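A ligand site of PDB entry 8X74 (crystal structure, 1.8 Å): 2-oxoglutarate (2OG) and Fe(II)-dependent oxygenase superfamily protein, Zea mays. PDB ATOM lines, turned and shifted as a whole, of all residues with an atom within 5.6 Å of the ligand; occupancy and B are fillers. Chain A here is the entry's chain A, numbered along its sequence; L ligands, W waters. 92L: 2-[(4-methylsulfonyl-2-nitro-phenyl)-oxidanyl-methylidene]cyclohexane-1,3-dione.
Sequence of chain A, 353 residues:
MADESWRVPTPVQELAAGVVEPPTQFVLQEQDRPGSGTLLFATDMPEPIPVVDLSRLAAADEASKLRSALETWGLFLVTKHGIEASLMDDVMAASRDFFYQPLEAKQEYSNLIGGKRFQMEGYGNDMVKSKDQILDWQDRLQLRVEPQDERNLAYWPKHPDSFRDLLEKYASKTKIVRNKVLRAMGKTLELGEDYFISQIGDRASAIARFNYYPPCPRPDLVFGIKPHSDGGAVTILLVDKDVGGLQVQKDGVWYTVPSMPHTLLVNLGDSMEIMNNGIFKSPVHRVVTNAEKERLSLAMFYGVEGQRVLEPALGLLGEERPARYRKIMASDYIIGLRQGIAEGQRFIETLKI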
ATOM      1  N   GLN A 142      -8.958  22.323  18.962  1.00  0.00           N
ATOM      2  CA  GLN A 142      -8.695  22.839  17.634  1.00  0.00           C
ATOM      3  C   GLN A 142      -8.330  24.316  17.726  1.00  0.00           C
ATOM      4  O   GLN A 142      -9.045  25.102  18.357  1.00  0.00           O
ATOM      5  CB  GLN A 142      -9.907  22.610  16.714  1.00  0.00           C
ATOM      6  CG  GLN A 142      -9.619  22.879  15.236  1.00  0.00           C
ATOM      7  CD  GLN A 142     -10.522  22.090  14.305  1.00  0.00           C
ATOM      8  OE1 GLN A 142     -10.738  20.888  14.488  1.00  0.00           O
ATOM      9  NE2 GLN A 142     -11.081  22.777  13.329  1.00  0.00           N
ATOM     10  N   ARG A 144      -6.507  27.872  15.719  1.00  0.00           N
ATOM     11  CA  ARG A 144      -5.954  28.609  14.579  1.00  0.00           C
ATOM     12  C   ARG A 144      -4.469  28.904  14.837  1.00  0.00           C
ATOM     13  O   ARG A 144      -4.110  29.526  15.844  1.00  0.00           O
ATOM     14  CB  ARG A 144      -6.750  29.907  14.375  1.00  0.00           C
ATOM     15  CG  ARG A 144      -5.971  30.985  13.630  1.00  0.00           C
ATOM     16  CD  ARG A 144      -6.099  30.841  12.146  1.00  0.00           C
ATOM     17  NE  ARG A 144      -7.487  30.795  11.685  1.00  0.00           N
ATOM     18  CZ  ARG A 144      -7.831  30.402  10.467  1.00  0.00           C
ATOM     19  NH1 ARG A 144      -6.872  30.028   9.619  1.00  0.00           N
ATOM     20  NH2 ARG A 144      -9.109  30.343  10.091  1.00  0.00           N
ATOM     21  N   GLU A 146      -2.146  29.705  11.853  1.00  0.00           N
ATOM     22  CA  GLU A 146      -1.789  30.768  10.892  1.00  0.00           C
ATOM     23  C   GLU A 146      -3.010  31.140  10.062  1.00  0.00           C
ATOM     24  O   GLU A 146      -3.874  30.301   9.805  1.00  0.00           O
ATOM     25  CB  GLU A 146      -0.619  30.333   9.985  1.00  0.00           C
ATOM     26  CG  GLU A 146       0.716  30.352  10.739  1.00  0.00           C
ATOM     27  CD  GLU A 146       1.845  29.646  10.030  1.00  0.00           C
ATOM     28  OE1 GLU A 146       1.569  28.781   9.173  1.00  0.00           O
ATOM     29  OE2 GLU A 146       3.026  29.962  10.340  1.00  0.00           O
ATOM     30  N   PRO A 147      -3.100  32.421   9.623  1.00  0.00           N
ATOM     31  CA  PRO A 147      -2.137  33.511   9.835  1.00  0.00           C
ATOM     32  C   PRO A 147      -1.966  33.857  11.311  1.00  0.00           C
ATOM     33  O   PRO A 147      -2.933  33.824  12.072  1.00  0.00           O
ATOM     34  CB  PRO A 147      -2.761  34.688   9.067  1.00  0.00           C
ATOM     35  CG  PRO A 147      -3.764  34.072   8.130  1.00  0.00           C
ATOM     36  CD  PRO A 147      -4.289  32.868   8.878  1.00  0.00           C
ATOM     37  N   GLU A 150      -4.280  36.071  13.213  1.00  0.00           N
ATOM     38  CA  GLU A 150      -5.652  35.635  13.471  1.00  0.00           C
ATOM     39  C   GLU A 150      -5.751  34.667  14.644  1.00  0.00           C
ATOM     40  O   GLU A 150      -6.853  34.221  14.963  1.00  0.00           O
ATOM     41  CB  GLU A 150      -6.255  34.991  12.222  1.00  0.00           C
ATOM     42  CG  GLU A 150      -6.485  35.979  11.086  1.00  0.00           C
ATOM     43  CD  GLU A 150      -6.956  35.307   9.829  1.00  0.00           C
ATOM     44  OE1 GLU A 150      -6.782  35.887   8.745  1.00  0.00           O
ATOM     45  OE2 GLU A 150      -7.485  34.175   9.895  1.00  0.00           O
ATOM     46  N   SER A 205      -3.165  29.512   5.436  1.00  0.00           N
ATOM     47  CA  SER A 205      -3.832  29.183   6.682  1.00  0.00           C
ATOM     48  C   SER A 205      -3.277  27.904   7.291  1.00  0.00           C
ATOM     49  O   SER A 205      -2.825  27.000   6.582  1.00  0.00           O
ATOM     50  CB  SER A 205      -5.307  29.006   6.438  1.00  0.00           C
ATOM     51  OG  SER A 205      -5.465  28.158   5.300  1.00  0.00           O
ATOM     52  N   ALA A 206      -3.352  27.810   8.612  1.00  0.00           N
ATOM     53  CA  ALA A 206      -2.908  26.604   9.288  1.00  0.00           C
ATOM     54  C   ALA A 206      -3.754  26.431  10.532  1.00  0.00           C
ATOM     55  O   ALA A 206      -3.862  27.348  11.335  1.00  0.00           O
ATOM     56  CB  ALA A 206      -1.424  26.656   9.674  1.00  0.00           C
ATOM     57  N   ILE A 207      -4.340  25.239  10.675  1.00  0.00           N
ATOM     58  CA  ILE A 207      -5.153  24.923  11.831  1.00  0.00           C
ATOM     59  C   ILE A 207      -4.584  23.662  12.462  1.00  0.00           C
ATOM     60  O   ILE A 207      -4.282  22.694  11.759  1.00  0.00           O
ATOM     61  CB  ILE A 207      -6.622  24.704  11.467  1.00  0.00           C
ATOM     62  CG1 ILE A 207      -7.267  26.048  11.102  1.00  0.00           C
ATOM     63  CG2 ILE A 207      -7.369  24.029  12.624  1.00  0.00           C
ATOM     64  CD1 ILE A 207      -8.727  25.917  10.781  1.00  0.00           C
ATOM     65  N   SER A 229     -13.355  13.681   4.159  1.00  0.00           N
ATOM     66  CA  SER A 229     -12.126  14.216   3.585  1.00  0.00           C
ATOM     67  C   SER A 229     -11.828  15.572   4.225  1.00  0.00           C
ATOM     68  O   SER A 229     -12.744  16.273   4.678  1.00  0.00           O
ATOM     69  CB  SER A 229     -12.195  14.335   2.057  1.00  0.00           C
ATOM     70  OG  SER A 229     -13.316  15.109   1.636  1.00  0.00           O
ATOM     71  N   ASP A 230     -10.550  15.917   4.304  1.00  0.00           N
ATOM     72  CA  ASP A 230     -10.208  17.196   4.912  1.00  0.00           C
ATOM     73  C   ASP A 230     -10.435  18.322   3.900  1.00  0.00           C
ATOM     74  O   ASP A 230     -10.433  18.111   2.689  1.00  0.00           O
ATOM     75  CB  ASP A 230      -8.738  17.231   5.344  1.00  0.00           C
ATOM     76  CG  ASP A 230      -8.390  16.181   6.341  1.00  0.00           C
ATOM     77  OD1 ASP A 230      -9.287  15.705   7.063  1.00  0.00           O
ATOM     78  OD2 ASP A 230      -7.197  15.853   6.428  1.00  0.00           O
ATOM     79  N   GLY A 231     -10.637  19.538   4.422  1.00  0.00           N
ATOM     80  CA  GLY A 231     -11.035  20.630   3.551  1.00  0.00           C
ATOM     81  C   GLY A 231      -9.932  21.469   2.931  1.00  0.00           C
ATOM     82  O   GLY A 231     -10.190  22.199   1.956  1.00  0.00           O
ATOM     83  N   GLY A 232      -8.722  21.405   3.462  1.00  0.00           N
ATOM     84  CA  GLY A 232      -7.640  22.291   3.063  1.00  0.00           C
ATOM     85  C   GLY A 232      -6.878  21.785   1.858  1.00  0.00           C
ATOM     86  O   GLY A 232      -7.374  20.983   1.071  1.00  0.00           O
ATOM     87  N   ALA A 233      -5.638  22.266   1.718  1.00  0.00           N
ATOM     88  CA  ALA A 233      -4.780  21.821   0.622  1.00  0.00           C
ATOM     89  C   ALA A 233      -4.049  20.515   0.960  1.00  0.00           C
ATOM     90  O   ALA A 233      -4.123  19.530   0.203  1.00  0.00           O
ATOM     91  CB  ALA A 233      -3.771  22.917   0.261  1.00  0.00           C
ATOM     92  N   VAL A 234      -3.323  20.480   2.083  1.00  0.00           N
ATOM     93  CA  VAL A 234      -2.675  19.263   2.544  1.00  0.00           C
ATOM     94  C   VAL A 234      -2.828  19.206   4.053  1.00  0.00           C
ATOM     95  O   VAL A 234      -2.935  20.245   4.713  1.00  0.00           O
ATOM     96  CB  VAL A 234      -1.181  19.169   2.155  1.00  0.00           C
ATOM     97  CG1 VAL A 234      -0.991  19.026   0.632  1.00  0.00           C
ATOM     98  CG2 VAL A 234      -0.412  20.363   2.685  1.00  0.00           C
ATOM     99  N   THR A 235      -2.834  17.996   4.593  1.00  0.00           N
ATOM    100  CA  THR A 235      -2.857  17.774   6.037  1.00  0.00           C
ATOM    101  C   THR A 235      -1.601  16.996   6.383  1.00  0.00           C
ATOM    102  O   THR A 235      -1.250  16.027   5.697  1.00  0.00           O
ATOM    103  CB  THR A 235      -4.100  16.968   6.455  1.00  0.00           C
ATOM    104  OG1 THR A 235      -5.280  17.683   6.088  1.00  0.00           O
ATOM    105  CG2 THR A 235      -4.115  16.644   7.952  1.00  0.00           C
ATOM    106  N   SER A 271      -9.441  21.295  -1.021  1.00  0.00           N
ATOM    107  CA  SER A 271      -9.000  22.469  -1.761  1.00  0.00           C
ATOM    108  C   SER A 271      -8.019  22.079  -2.860  1.00  0.00           C
ATOM    109  O   SER A 271      -8.040  22.644  -3.952  1.00  0.00           O
ATOM    110  CB  SER A 271      -8.375  23.480  -0.812  1.00  0.00           C
ATOM    111  OG  SER A 271      -9.345  23.937   0.109  1.00  0.00           O
ATOM    112  N   PHE A 301      -3.703  21.130   9.491  1.00  0.00           N
ATOM    113  CA  PHE A 301      -4.401  21.413   8.246  1.00  0.00           C
ATOM    114  C   PHE A 301      -3.808  22.664   7.618  1.00  0.00           C
ATOM    115  O   PHE A 301      -3.809  23.714   8.252  1.00  0.00           O
ATOM    116  CB  PHE A 301      -5.899  21.625   8.479  1.00  0.00           C
ATOM    117  CG  PHE A 301      -6.577  20.490   9.186  1.00  0.00           C
ATOM    118  CD1 PHE A 301      -6.692  19.243   8.588  1.00  0.00           C
ATOM    119  CD2 PHE A 301      -7.116  20.678  10.443  1.00  0.00           C
ATOM    120  CE1 PHE A 301      -7.336  18.201   9.255  1.00  0.00           C
ATOM    121  CE2 PHE A 301      -7.752  19.631  11.108  1.00  0.00           C
ATOM    122  CZ  PHE A 301      -7.870  18.397  10.516  1.00  0.00           C
ATOM    123  N   TYR A 302      -3.301  22.555   6.396  1.00  0.00           N
ATOM    124  CA  TYR A 302      -2.757  23.698   5.688  1.00  0.00           C
ATOM    125  C   TYR A 302      -3.636  23.996   4.484  1.00  0.00           C
ATOM    126  O   TYR A 302      -3.918  23.105   3.680  1.00  0.00           O
ATOM    127  CB  TYR A 302      -1.313  23.430   5.220  1.00  0.00           C
ATOM    128  CG  TYR A 302      -0.312  23.514   6.356  1.00  0.00           C
ATOM    129  CD1 TYR A 302       0.063  24.747   6.891  1.00  0.00           C
ATOM    130  CD2 TYR A 302       0.247  22.364   6.894  1.00  0.00           C
ATOM    131  CE1 TYR A 302       0.982  24.833   7.929  1.00  0.00           C
ATOM    132  CE2 TYR A 302       1.169  22.433   7.936  1.00  0.00           C
ATOM    133  CZ  TYR A 302       1.524  23.677   8.451  1.00  0.00           C
ATOM    134  OH  TYR A 302       2.444  23.768   9.480  1.00  0.00           O
ATOM    135  N   GLY A 303      -4.088  25.243   4.375  1.00  0.00           N
ATOM    136  CA  GLY A 303      -5.018  25.633   3.344  1.00  0.00           C
ATOM    137  C   GLY A 303      -4.567  26.911   2.667  1.00  0.00           C
ATOM    138  O   GLY A 303      -3.554  27.511   3.038  1.00  0.00           O
ATOM    139  N   VAL A 304      -5.346  27.311   1.681  1.00  0.00           N
ATOM    140  CA  VAL A 304      -5.051  28.562   0.994  1.00  0.00           C
ATOM    141  C   VAL A 304      -5.608  29.725   1.805  1.00  0.00           C
ATOM    142  O   VAL A 304      -6.449  29.558   2.684  1.00  0.00           O
ATOM    143  CB  VAL A 304      -5.611  28.561  -0.440  1.00  0.00           C
ATOM    144  CG1 VAL A 304      -5.053  27.373  -1.230  1.00  0.00           C
ATOM    145  CG2 VAL A 304      -7.097  28.472  -0.385  1.00  0.00           C
ATOM    146  N   GLU A 305      -5.130  30.933   1.501  1.00  0.00           N
ATOM    147  CA  GLU A 305      -5.649  32.093   2.203  1.00  0.00           C
ATOM    148  C   GLU A 305      -7.140  32.276   1.897  1.00  0.00           C
ATOM    149  O   GLU A 305      -7.639  31.819   0.875  1.00  0.00           O
ATOM    150  CB  GLU A 305      -4.842  33.347   1.838  1.00  0.00           C
ATOM    151  CG  GLU A 305      -4.937  33.773   0.378  1.00  0.00           C
ATOM    152  CD  GLU A 305      -4.035  34.944   0.029  1.00  0.00           C
ATOM    153  OE1 GLU A 305      -3.169  35.347   0.846  1.00  0.00           O
ATOM    154  OE2 GLU A 305      -4.184  35.457  -1.105  1.00  0.00           O
ATOM    155  N   GLY A 306      -7.854  32.919   2.828  1.00  0.00           N
ATOM    156  CA  GLY A 306      -9.301  32.924   2.787  1.00  0.00           C
ATOM    157  C   GLY A 306      -9.906  33.503   1.518  1.00  0.00           C
ATOM    158  O   GLY A 306     -10.949  33.041   1.054  1.00  0.00           O
ATOM    159  N   ALA A 330     -12.179  30.302  -1.202  1.00  0.00           N
ATOM    160  CA  ALA A 330     -11.770  29.336  -0.190  1.00  0.00           C
ATOM    161  C   ALA A 330     -12.616  29.429   1.072  1.00  0.00           C
ATOM    162  O   ALA A 330     -13.012  28.401   1.642  1.00  0.00           O
ATOM    163  CB  ALA A 330     -10.292  29.534   0.155  1.00  0.00           C
ATOM    164  N   SER A 331     -12.895  30.646   1.541  1.00  0.00           N
ATOM    165  CA  SER A 331     -13.677  30.800   2.762  1.00  0.00           C
ATOM    166  C   SER A 331     -15.091  30.262   2.573  1.00  0.00           C
ATOM    167  O   SER A 331     -15.651  29.638   3.476  1.00  0.00           O
ATOM    168  CB  SER A 331     -13.712  32.264   3.168  1.00  0.00           C
ATOM    169  OG  SER A 331     -13.954  33.101   2.058  1.00  0.00           O
ATOM    170  N   ILE A 334     -15.011  26.401   2.841  1.00  0.00           N
ATOM    171  CA  ILE A 334     -14.925  25.901   4.208  1.00  0.00           C
ATOM    172  C   ILE A 334     -16.261  26.027   4.923  1.00  0.00           C
ATOM    173  O   ILE A 334     -16.689  25.111   5.633  1.00  0.00           O
ATOM    174  CB  ILE A 334     -13.803  26.632   4.970  1.00  0.00           C
ATOM    175  CG1 ILE A 334     -12.432  26.209   4.440  1.00  0.00           C
ATOM    176  CG2 ILE A 334     -13.919  26.391   6.483  1.00  0.00           C
ATOM    177  CD1 ILE A 334     -12.260  24.720   4.272  1.00  0.00           C
ATOM    178  N   LEU A 337     -18.533  23.449   3.591  1.00  0.00           N
ATOM    179  CA  LEU A 337     -18.100  22.151   3.997  1.00  0.00           C
ATOM    180  C   LEU A 337     -18.640  21.831   5.364  1.00  0.00           C
ATOM    181  O   LEU A 337     -18.831  20.694   5.705  1.00  0.00           O
ATOM    182  CB  LEU A 337     -16.578  22.058   4.015  1.00  0.00           C
ATOM    183  CG  LEU A 337     -15.910  20.768   4.420  1.00  0.00           C
ATOM    184  CD1 LEU A 337     -16.186  19.661   3.456  1.00  0.00           C
ATOM    185  CD2 LEU A 337     -14.423  20.877   4.610  1.00  0.00           C
HETATM  186  C10 92L L   1     -10.924  24.341   7.754  1.00  0.00           C
HETATM  187  C13 92L L   1      -8.335  24.653   6.914  1.00  0.00           C
HETATM  188  C1  92L L   1      -9.773  28.120   3.580  1.00  0.00           C
HETATM  189  C2  92L L   1      -9.938  29.628   3.801  1.00  0.00           C
HETATM  190  C3  92L L   1     -10.025  30.009   5.274  1.00  0.00           C
HETATM  191  C4  92L L   1      -8.752  29.575   5.991  1.00  0.00           C
HETATM  192  C5  92L L   1      -8.387  28.065   5.804  1.00  0.00           C
HETATM  193  C6  92L L   1      -8.657  27.479   4.401  1.00  0.00           C
HETATM  194  C7  92L L   1      -8.457  27.176   7.108  1.00  0.00           C
HETATM  195  C8  92L L   1      -9.102  25.790   7.194  1.00  0.00           C
HETATM  196  C9  92L L   1     -10.399  25.623   7.637  1.00  0.00           C
HETATM  197  C11 92L L   1     -10.156  23.234   7.443  1.00  0.00           C
HETATM  198  C12 92L L   1      -8.854  23.383   7.026  1.00  0.00           C
HETATM  199  O14 92L L   1      -8.744  26.079   4.414  1.00  0.00           O
HETATM  200  O15 92L L   1      -8.723  29.947   7.350  1.00  0.00           O
HETATM  201  O16 92L L   1      -8.752  27.912   8.258  1.00  0.00           O
HETATM  202  N17 92L L   1      -6.969  24.777   6.470  1.00  0.00           N
HETATM  203  O18 92L L   1      -6.354  23.678   5.876  1.00  0.00           O
HETATM  204  O19 92L L   1      -6.229  25.955   6.641  1.00  0.00           O
HETATM  205  S20 92L L   1     -10.844  21.562   7.620  1.00  0.00           S
HETATM  206  O21 92L L   1     -12.394  21.509   7.102  1.00  0.00           O
HETATM  207  O22 92L L   1      -9.898  20.456   6.872  1.00  0.00           O
HETATM  208  C23 92L L   1     -10.842  21.112   9.392  1.00  0.00           C
HETATM  209  O   HOH W   1      -7.835  32.490   7.197  1.00  0.00           O
HETATM  210  O   HOH W   2     -12.293  29.701   7.790  1.00  0.00           O
HETATM  211  O   HOH W   3      -7.847  25.700   1.855  1.00  0.00           O
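The guanidinium group (NH2) of Arg 144 sits at hydrogen-bond distance from an oxygen (O15) of the ligand, 2.8 Å away.
The backbone NH (N) of Gly 231 is in hydrogen-bond range of an oxygen (O22) of the ligand, 2.7 Å away.
An oxygen (O18) of the ligand lies within hydrogen-bond range of the backbone NH (N) of Gly 303, 3.1 Å away.
The side-chain hydroxyl (OG) of Ser 205 lies within hydrogen-bond range of an oxygen (O19) of the ligand.
The backbone NH (N) of Tyr 302 sits close to an oxygen (O18) of the ligand, at 3.3 Å.
The backbone carbonyl oxygen (O) of Tyr 302 is in hydrogen-bond range of the backbone NH (N) of Ala 233 (2.7 Å).
The backbone carbonyl oxygen of Ile 207 is in hydrogen-bond range of the backbone NH of Phe 301, at 2.8 Å.
OD2 of Asp 230 sits at hydrogen-bond distance from OG1 of Thr 235, 2.7 Å away.
The backbone carbonyl oxygen (O) of Gly 232 is in hydrogen-bond range of the backbone NH (N) of Ser 271.
O of Gly 306 is in hydrogen-bond range of N of Ser 331 (3.1 Å).
NH1 of Arg 144 lies within hydrogen-bond range of O of Glu 146, at 3.0 Å.
O of Glu 146 sits at hydrogen-bond distance from N of Ala 206 (2.8 Å).
NE of Arg 144 lies within salt-bridge range of OE2 of Glu 150 (3.8 Å).
An oxygen (O18) of the ligand sits close to the backbone carbonyl oxygen (O) of Phe 301 (3.5 Å).
N of Ala 206 touches O19 of the ligand, 3.95 Å away.
Ile 207 touches the ligand.
Asp 230 touches the ligand.
Gly 232 touches the ligand.
Val 304 touches the ligand.
Gly 306 touches the ligand (CA to C2, 3.5 Å).
CB of Ala 330 touches C2 of the ligand (3.7 Å).
Ser 331 touches the ligand.
Ile 334 touches the ligand (CG1 to C1, 3.4 Å).
CD2 of Leu 337 touches O21 of the ligand, at 3.3 Å.
Within 4 Å of the ligand: Arg 144, Ser 205, Ala 206, Ile 207, Asp 230, Gly 231, Gly 232, Phe 301, Tyr 302, Gly 303, Val 304, Gly 306, Ala 330, Ser 331, Ile 334 and Leu 337.
Water W1 lies within hydrogen-bond range of an oxygen (O15) of the ligand (2.7 Å) and the side-chain carboxylate (OE2) of Glu 150 (3.2 Å).
Water W3 lies within hydrogen-bond range of an oxygen (O14) of the ligand (2.7 Å), the side-chain hydroxyl (OG) of Ser 271 (2.9 Å) and the backbone NH (N) of Val 304 (3.0 Å).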
